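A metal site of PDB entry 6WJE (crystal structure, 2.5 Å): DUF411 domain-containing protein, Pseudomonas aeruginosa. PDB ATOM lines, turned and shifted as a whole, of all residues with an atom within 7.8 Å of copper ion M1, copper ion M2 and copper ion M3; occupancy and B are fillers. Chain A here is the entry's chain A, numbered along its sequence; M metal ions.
A ring nitrogen (ND1) of His 67 is in hydrogen-bond range of the backbone carbonyl oxygen of Pro 95. A ring nitrogen (NE2) of His 55 lies within hydrogen-bond range of the backbone carbonyl oxygen of Gly 66 (2.7 Å). SG of Cys 16 is disulfide-bonded to SG of Cys 13. The side-chain sulfur of Cys 15 lies close to the side-chain sulfur of Cys 13.
Merely in contact with copper ion M1: Cys 13 (3.7 Å). Within 4 Å of copper ion M1: Cys 13, Cys 16, Cys 54, His 55 and His 67. The nearest printed residue that does not touch copper ion M1 is Cys 15 (4.5 Å).
Merely in contact with copper ion M2: Cys 13 (3.9 Å). Six residues have an atom within 4 Å of copper ion M2: Cys 13, Cys 15, Cys 16, Cys 54, His 67 and Met 90. The nearest printed residue that does not touch copper ion M2 is Met 97 (4.3 Å).
Of the 29 residues printed, 3 come within 4 Å of copper ion M3.
Copper ion M1 is bound by ND1 of His 55 (2.1 Å), SG of Cys 54 (2.1 Å) and SG of Cys 16 (2.2 Å). Copper ion M1 has three donor atoms within binding distance.
Copper ion M2 is bound by a ring nitrogen (NE2) of His 67 (2.0 Å), the side-chain sulfur of Cys 54 (2.2 Å) and the side-chain sulfur of Cys 15 (2.2 Å).
SD of Met 97 binds copper ion M3. Copper ion M3 is bound by SG of Cys 15, at 2.4 Å. Copper ion M3 is bound by the side-chain sulfur (SD) of Met 90 (2.4 Å). Copper ion M3 has three donor atoms within binding distance.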
ATOM      1  N   VAL A   7     -26.834  33.887  21.442  1.00  0.00           N
ATOM      2  CA  VAL A   7     -26.807  32.820  20.448  1.00  0.00           C
ATOM      3  C   VAL A   7     -27.531  31.597  21.005  1.00  0.00           C
ATOM      4  O   VAL A   7     -27.311  31.236  22.167  1.00  0.00           O
ATOM      5  CB  VAL A   7     -25.365  32.476  20.024  1.00  0.00           C
ATOM      6  CG1 VAL A   7     -25.335  31.344  19.001  1.00  0.00           C
ATOM      7  CG2 VAL A   7     -24.741  33.716  19.418  1.00  0.00           C
ATOM      8  N   HIS A   8     -28.435  31.017  20.213  1.00  0.00           N
ATOM      9  CA  HIS A   8     -29.042  29.729  20.515  1.00  0.00           C
ATOM     10  C   HIS A   8     -28.523  28.732  19.490  1.00  0.00           C
ATOM     11  O   HIS A   8     -28.440  29.044  18.290  1.00  0.00           O
ATOM     12  CB  HIS A   8     -30.614  29.733  20.469  1.00  0.00           C
ATOM     13  CG  HIS A   8     -31.287  30.617  21.516  1.00  0.00           C
ATOM     14  ND1 HIS A   8     -32.184  30.150  22.478  1.00  0.00           N
ATOM     15  CD2 HIS A   8     -31.206  31.946  21.706  1.00  0.00           C
ATOM     16  CE1 HIS A   8     -32.585  31.165  23.220  1.00  0.00           C
ATOM     17  NE2 HIS A   8     -32.013  32.262  22.761  1.00  0.00           N
ATOM     18  N   ARG A   9     -28.169  27.532  19.934  1.00  0.00           N
ATOM     19  CA  ARG A   9     -27.663  26.506  19.036  1.00  0.00           C
ATOM     20  C   ARG A   9     -27.813  25.156  19.701  1.00  0.00           C
ATOM     21  O   ARG A   9     -28.014  25.047  20.911  1.00  0.00           O
ATOM     22  CB  ARG A   9     -26.207  26.756  18.647  1.00  0.00           C
ATOM     23  CG  ARG A   9     -25.317  27.046  19.811  1.00  0.00           C
ATOM     24  CD  ARG A   9     -24.574  25.851  20.161  1.00  0.00           C
ATOM     25  NE  ARG A   9     -23.688  26.071  21.288  1.00  0.00           N
ATOM     26  CZ  ARG A   9     -23.078  25.073  21.945  1.00  0.00           C
ATOM     27  NH1 ARG A   9     -23.285  23.809  21.566  1.00  0.00           N
ATOM     28  NH2 ARG A   9     -22.274  25.342  22.961  1.00  0.00           N
ATOM     29  N   ASP A  10     -27.694  24.114  18.876  1.00  0.00           N
ATOM     30  CA  ASP A  10     -27.743  22.737  19.343  1.00  0.00           C
ATOM     31  C   ASP A  10     -26.460  22.324  20.072  1.00  0.00           C
ATOM     32  O   ASP A  10     -25.362  22.841  19.816  1.00  0.00           O
ATOM     33  CB  ASP A  10     -28.004  21.830  18.133  1.00  0.00           C
ATOM     34  CG  ASP A  10     -28.135  20.366  18.493  1.00  0.00           C
ATOM     35  OD1 ASP A  10     -29.244  19.944  18.920  1.00  0.00           O
ATOM     36  OD2 ASP A  10     -27.127  19.637  18.323  1.00  0.00           O
ATOM     37  N   CYS A  13     -23.399  21.131  17.832  1.00  0.00           N
ATOM     38  CA  CYS A  13     -23.049  21.969  16.665  1.00  0.00           C
ATOM     39  C   CYS A  13     -21.697  22.573  16.966  1.00  0.00           C
ATOM     40  O   CYS A  13     -21.592  23.632  17.585  1.00  0.00           O
ATOM     41  CB  CYS A  13     -24.091  23.042  16.337  1.00  0.00           C
ATOM     42  SG  CYS A  13     -23.693  24.038  14.761  1.00  0.00           S
ATOM     43  N   GLY A  14     -20.667  21.895  16.493  1.00  0.00           N
ATOM     44  CA  GLY A  14     -19.324  22.330  16.714  1.00  0.00           C
ATOM     45  C   GLY A  14     -18.912  23.530  15.883  1.00  0.00           C
ATOM     46  O   GLY A  14     -18.201  24.385  16.396  1.00  0.00           O
ATOM     47  N   CYS A  15     -19.255  23.564  14.591  1.00  0.00           N
ATOM     48  CA  CYS A  15     -19.051  24.803  13.861  1.00  0.00           C
ATOM     49  C   CYS A  15     -19.653  25.987  14.599  1.00  0.00           C
ATOM     50  O   CYS A  15     -18.989  27.022  14.747  1.00  0.00           O
ATOM     51  CB  CYS A  15     -19.551  24.684  12.406  1.00  0.00           C
ATOM     52  SG  CYS A  15     -21.317  24.283  12.223  1.00  0.00           S
ATOM     53  N   CYS A  16     -20.877  25.839  15.100  1.00  0.00           N
ATOM     54  CA  CYS A  16     -21.513  26.924  15.859  1.00  0.00           C
ATOM     55  C   CYS A  16     -20.655  27.374  17.039  1.00  0.00           C
ATOM     56  O   CYS A  16     -20.558  28.580  17.313  1.00  0.00           O
ATOM     57  CB  CYS A  16     -22.903  26.516  16.373  1.00  0.00           C
ATOM     58  SG  CYS A  16     -24.078  26.036  15.068  1.00  0.00           S
ATOM     59  N   LYS A  17     -19.999  26.431  17.738  1.00  0.00           N
ATOM     60  CA  LYS A  17     -19.124  26.831  18.826  1.00  0.00           C
ATOM     61  C   LYS A  17     -17.905  27.584  18.309  1.00  0.00           C
ATOM     62  O   LYS A  17     -17.444  28.547  18.939  1.00  0.00           O
ATOM     63  CB  LYS A  17     -18.662  25.628  19.630  1.00  0.00           C
ATOM     64  CG  LYS A  17     -19.692  24.867  20.435  1.00  0.00           C
ATOM     65  CD  LYS A  17     -19.019  23.590  21.018  1.00  0.00           C
ATOM     66  CE  LYS A  17     -19.992  22.586  21.643  1.00  0.00           C
ATOM     67  N   ASP A  18     -17.404  27.153  17.149  1.00  0.00           N
ATOM     68  CA  ASP A  18     -16.208  27.806  16.518  1.00  0.00           C
ATOM     69  C   ASP A  18     -16.548  29.273  16.211  1.00  0.00           C
ATOM     70  O   ASP A  18     -15.711  30.138  16.511  1.00  0.00           O
ATOM     71  CB  ASP A  18     -15.778  27.043  15.262  1.00  0.00           C
ATOM     72  CG  ASP A  18     -14.442  27.510  14.707  1.00  0.00           C
ATOM     73  OD1 ASP A  18     -13.633  28.058  15.492  1.00  0.00           O
ATOM     74  OD2 ASP A  18     -14.219  27.342  13.494  1.00  0.00           O
ATOM     75  N   TRP A  19     -17.727  29.509  15.634  1.00  0.00           N
ATOM     76  CA  TRP A  19     -18.186  30.855  15.284  1.00  0.00           C
ATOM     77  C   TRP A  19     -18.261  31.753  16.510  1.00  0.00           C
ATOM     78  O   TRP A  19     -17.816  32.902  16.463  1.00  0.00           O
ATOM     79  CB  TRP A  19     -19.552  30.772  14.592  1.00  0.00           C
ATOM     80  CG  TRP A  19     -20.177  32.090  14.158  1.00  0.00           C
ATOM     81  CD1 TRP A  19     -19.801  32.857  13.075  1.00  0.00           C
ATOM     82  CD2 TRP A  19     -21.283  32.778  14.753  1.00  0.00           C
ATOM     83  NE1 TRP A  19     -20.612  33.959  12.964  1.00  0.00           N
ATOM     84  CE2 TRP A  19     -21.523  33.937  13.996  1.00  0.00           C
ATOM     85  CE3 TRP A  19     -22.098  32.504  15.851  1.00  0.00           C
ATOM     86  CZ2 TRP A  19     -22.552  34.835  14.295  1.00  0.00           C
ATOM     87  CZ3 TRP A  19     -23.120  33.394  16.165  1.00  0.00           C
ATOM     88  CH2 TRP A  19     -23.331  34.554  15.387  1.00  0.00           C
ATOM     89  N   LYS A  42     -36.103  30.287  15.329  1.00  0.00           N
ATOM     90  CA  LYS A  42     -36.138  30.939  14.021  1.00  0.00           C
ATOM     91  C   LYS A  42     -37.536  31.457  13.717  1.00  0.00           C
ATOM     92  O   LYS A  42     -37.700  32.522  13.079  1.00  0.00           O
ATOM     93  CB  LYS A  42     -35.681  29.967  12.939  1.00  0.00           C
ATOM     94  CG  LYS A  42     -34.210  29.643  12.961  1.00  0.00           C
ATOM     95  CD  LYS A  42     -33.930  28.424  12.119  1.00  0.00           C
ATOM     96  CE  LYS A  42     -32.683  27.672  12.591  1.00  0.00           C
ATOM     97  NZ  LYS A  42     -31.464  28.550  12.655  1.00  0.00           N
ATOM     98  N   SER A  53     -30.136  28.269   8.775  1.00  0.00           N
ATOM     99  CA  SER A  53     -28.772  27.830   8.994  1.00  0.00           C
ATOM    100  C   SER A  53     -28.694  27.067  10.315  1.00  0.00           C
ATOM    101  O   SER A  53     -29.710  26.660  10.877  1.00  0.00           O
ATOM    102  CB  SER A  53     -27.814  29.026   8.987  1.00  0.00           C
ATOM    103  OG  SER A  53     -26.522  28.585   8.655  1.00  0.00           O
ATOM    104  N   CYS A  54     -27.467  26.811  10.771  1.00  0.00           N
ATOM    105  CA  CYS A  54     -27.173  25.990  11.941  1.00  0.00           C
ATOM    106  C   CYS A  54     -27.427  26.696  13.273  1.00  0.00           C
ATOM    107  O   CYS A  54     -27.489  26.015  14.291  1.00  0.00           O
ATOM    108  CB  CYS A  54     -25.741  25.468  11.898  1.00  0.00           C
ATOM    109  SG  CYS A  54     -24.526  26.676  11.478  1.00  0.00           S
ATOM    110  N   HIS A  55     -27.429  28.032  13.322  1.00  0.00           N
ATOM    111  CA  HIS A  55     -27.567  28.683  14.617  1.00  0.00           C
ATOM    112  C   HIS A  55     -28.278  30.001  14.360  1.00  0.00           C
ATOM    113  O   HIS A  55     -28.223  30.543  13.256  1.00  0.00           O
ATOM    114  CB  HIS A  55     -26.223  28.907  15.318  1.00  0.00           C
ATOM    115  CG  HIS A  55     -25.329  29.881  14.615  1.00  0.00           C
ATOM    116  ND1 HIS A  55     -24.193  29.507  13.917  1.00  0.00           N
ATOM    117  CD2 HIS A  55     -25.363  31.231  14.552  1.00  0.00           C
ATOM    118  CE1 HIS A  55     -23.612  30.572  13.401  1.00  0.00           C
ATOM    119  NE2 HIS A  55     -24.294  31.635  13.785  1.00  0.00           N
ATOM    120  N   THR A  56     -28.871  30.566  15.431  1.00  0.00           N
ATOM    121  CA  THR A  56     -29.581  31.841  15.358  1.00  0.00           C
ATOM    122  C   THR A  56     -29.175  32.746  16.503  1.00  0.00           C
ATOM    123  O   THR A  56     -29.389  32.410  17.675  1.00  0.00           O
ATOM    124  CB  THR A  56     -31.104  31.644  15.408  1.00  0.00           C
ATOM    125  OG1 THR A  56     -31.493  30.698  14.404  1.00  0.00           O
ATOM    126  CG2 THR A  56     -31.821  32.957  15.144  1.00  0.00           C
ATOM    127  N   GLU A  65     -28.432  35.076  11.389  1.00  0.00           N
ATOM    128  CA  GLU A  65     -28.639  33.677  11.029  1.00  0.00           C
ATOM    129  C   GLU A  65     -27.388  33.123  10.350  1.00  0.00           C
ATOM    130  O   GLU A  65     -27.049  33.532   9.234  1.00  0.00           O
ATOM    131  CB  GLU A  65     -29.834  33.511  10.109  1.00  0.00           C
ATOM    132  CG  GLU A  65     -30.097  32.046   9.819  1.00  0.00           C
ATOM    133  CD  GLU A  65     -30.827  31.322  10.969  1.00  0.00           C
ATOM    134  OE1 GLU A  65     -31.353  31.991  11.878  1.00  0.00           O
ATOM    135  OE2 GLU A  65     -30.852  30.068  10.970  1.00  0.00           O
ATOM    136  N   GLY A  66     -26.761  32.128  10.992  1.00  0.00           N
ATOM    137  CA  GLY A  66     -25.621  31.444  10.440  1.00  0.00           C
ATOM    138  C   GLY A  66     -24.303  32.180  10.651  1.00  0.00           C
ATOM    139  O   GLY A  66     -24.170  33.072  11.487  1.00  0.00           O
ATOM    140  N   HIS A  67     -23.321  31.776   9.848  1.00  0.00           N
ATOM    141  CA  HIS A  67     -21.912  32.150  10.033  1.00  0.00           C
ATOM    142  C   HIS A  67     -21.640  33.503   9.388  1.00  0.00           C
ATOM    143  O   HIS A  67     -20.880  33.616   8.423  1.00  0.00           O
ATOM    144  CB  HIS A  67     -21.003  31.080   9.443  1.00  0.00           C
ATOM    145  CG  HIS A  67     -21.027  29.801  10.208  1.00  0.00           C
ATOM    146  ND1 HIS A  67     -20.101  29.505  11.181  1.00  0.00           N
ATOM    147  CD2 HIS A  67     -21.945  28.803  10.239  1.00  0.00           C
ATOM    148  CE1 HIS A  67     -20.395  28.335  11.722  1.00  0.00           C
ATOM    149  NE2 HIS A  67     -21.519  27.890  11.174  1.00  0.00           N
ATOM    150  N   GLY A  89     -27.480  28.125   5.085  1.00  0.00           N
ATOM    151  CA  GLY A  89     -26.684  26.904   4.961  1.00  0.00           C
ATOM    152  C   GLY A  89     -25.392  26.984   5.752  1.00  0.00           C
ATOM    153  O   GLY A  89     -25.304  27.683   6.777  1.00  0.00           O
ATOM    154  N   MET A  90     -24.347  26.321   5.257  1.00  0.00           N
ATOM    155  CA  MET A  90     -23.049  26.247   5.948  1.00  0.00           C
ATOM    156  C   MET A  90     -21.895  26.286   4.950  1.00  0.00           C
ATOM    157  O   MET A  90     -21.176  25.307   4.779  1.00  0.00           O
ATOM    158  CB  MET A  90     -22.977  25.000   6.832  1.00  0.00           C
ATOM    159  CG  MET A  90     -23.760  25.131   8.133  1.00  0.00           C
ATOM    160  SD  MET A  90     -23.569  23.783   9.319  1.00  0.00           S
ATOM    161  CE  MET A  90     -23.196  22.452   8.185  1.00  0.00           C
ATOM    162  N   PRO A  91     -21.657  27.434   4.310  1.00  0.00           N
ATOM    163  CA  PRO A  91     -20.578  27.512   3.314  1.00  0.00           C
ATOM    164  C   PRO A  91     -19.203  27.333   3.946  1.00  0.00           C
ATOM    165  O   PRO A  91     -18.918  27.900   4.997  1.00  0.00           O
ATOM    166  CB  PRO A  91     -20.750  28.921   2.722  1.00  0.00           C
ATOM    167  CG  PRO A  91     -21.508  29.688   3.739  1.00  0.00           C
ATOM    168  CD  PRO A  91     -22.406  28.697   4.442  1.00  0.00           C
ATOM    169  N   VAL A  92     -18.384  26.467   3.344  1.00  0.00           N
ATOM    170  CA  VAL A  92     -17.024  26.263   3.849  1.00  0.00           C
ATOM    171  C   VAL A  92     -16.210  27.533   3.673  1.00  0.00           C
ATOM    172  O   VAL A  92     -16.193  28.149   2.591  1.00  0.00           O
ATOM    173  CB  VAL A  92     -16.384  25.058   3.153  1.00  0.00           C
ATOM    174  CG1 VAL A  92     -15.028  24.659   3.762  1.00  0.00           C
ATOM    175  CG2 VAL A  92     -17.321  23.892   3.267  1.00  0.00           C
ATOM    176  N   SER A  94     -16.594  30.207   5.649  1.00  0.00           N
ATOM    177  CA  SER A  94     -17.166  31.254   6.456  1.00  0.00           C
ATOM    178  C   SER A  94     -16.634  31.053   7.872  1.00  0.00           C
ATOM    179  O   SER A  94     -16.182  29.957   8.218  1.00  0.00           O
ATOM    180  CB  SER A  94     -18.689  31.236   6.417  1.00  0.00           C
ATOM    181  OG  SER A  94     -19.227  30.060   7.002  1.00  0.00           O
ATOM    182  N   PRO A  95     -16.647  32.095   8.703  1.00  0.00           N
ATOM    183  CA  PRO A  95     -16.016  31.985  10.027  1.00  0.00           C
ATOM    184  C   PRO A  95     -16.689  30.925  10.890  1.00  0.00           C
ATOM    185  O   PRO A  95     -17.909  30.921  11.054  1.00  0.00           O
ATOM    186  CB  PRO A  95     -16.198  33.391  10.616  1.00  0.00           C
ATOM    187  CG  PRO A  95     -16.511  34.275   9.475  1.00  0.00           C
ATOM    188  CD  PRO A  95     -17.171  33.449   8.438  1.00  0.00           C
ATOM    189  N   GLY A  96     -15.884  30.039  11.469  1.00  0.00           N
ATOM    190  CA  GLY A  96     -16.396  28.898  12.196  1.00  0.00           C
ATOM    191  C   GLY A  96     -16.677  27.696  11.337  1.00  0.00           C
ATOM    192  O   GLY A  96     -16.970  26.609  11.879  1.00  0.00           O
ATOM    193  N   MET A  97     -16.603  27.840  10.015  1.00  0.00           N
ATOM    194  CA  MET A  97     -16.763  26.737   9.085  1.00  0.00           C
ATOM    195  C   MET A  97     -15.503  26.532   8.240  1.00  0.00           C
ATOM    196  O   MET A  97     -15.540  25.893   7.180  1.00  0.00           O
ATOM    197  CB  MET A  97     -17.991  26.986   8.184  1.00  0.00           C
ATOM    198  CG  MET A  97     -19.322  26.388   8.724  1.00  0.00           C
ATOM    199  SD  MET A  97     -19.284  24.580   8.917  1.00  0.00           S
ATOM    200  CE  MET A  97     -19.147  23.962   7.247  1.00  0.00           C
ATOM    201  N   GLU A  98     -14.365  27.045   8.705  1.00  0.00           N
ATOM    202  CA  GLU A  98     -13.149  27.057   7.904  1.00  0.00           C
ATOM    203  C   GLU A  98     -12.517  25.658   7.864  1.00  0.00           C
ATOM    204  O   GLU A  98     -12.371  24.990   8.888  1.00  0.00           O
ATOM    205  CB  GLU A  98     -12.192  28.135   8.468  1.00  0.00           C
ATOM    206  CG  GLU A  98     -11.283  27.805   9.689  1.00  0.00           C
ATOM    207  CD  GLU A  98     -11.816  28.135  11.124  1.00  0.00           C
ATOM    208  OE1 GLU A  98     -12.961  28.603  11.356  1.00  0.00           O
ATOM    209  OE2 GLU A  98     -11.019  27.938  12.086  1.00  0.00           O
ATOM    210  N   MET A  99     -12.192  25.190   6.676  1.00  0.00           N
ATOM    211  CA  MET A  99     -11.722  23.822   6.524  1.00  0.00           C
ATOM    212  C   MET A  99     -10.592  23.772   5.504  1.00  0.00           C
ATOM    213  O   MET A  99     -10.579  22.961   4.576  1.00  0.00           O
ATOM    214  CB  MET A  99     -12.874  22.915   6.147  1.00  0.00           C
ATOM    215  CG  MET A  99     -13.456  22.217   7.311  1.00  0.00           C
ATOM    216  SD  MET A  99     -15.042  21.607   6.791  1.00  0.00           S
ATOM    217  CE  MET A  99     -16.034  22.483   7.967  1.00  0.00           C
HETATM  218 CU    CU M   1     -24.204  27.451  13.422  1.00  0.00          CU
HETATM  219 CU    CU M   2     -22.446  26.145  11.706  1.00  0.00          CU
HETATM  220 CU    CU M   3     -21.221  23.733   9.904  1.00  0.00          CU
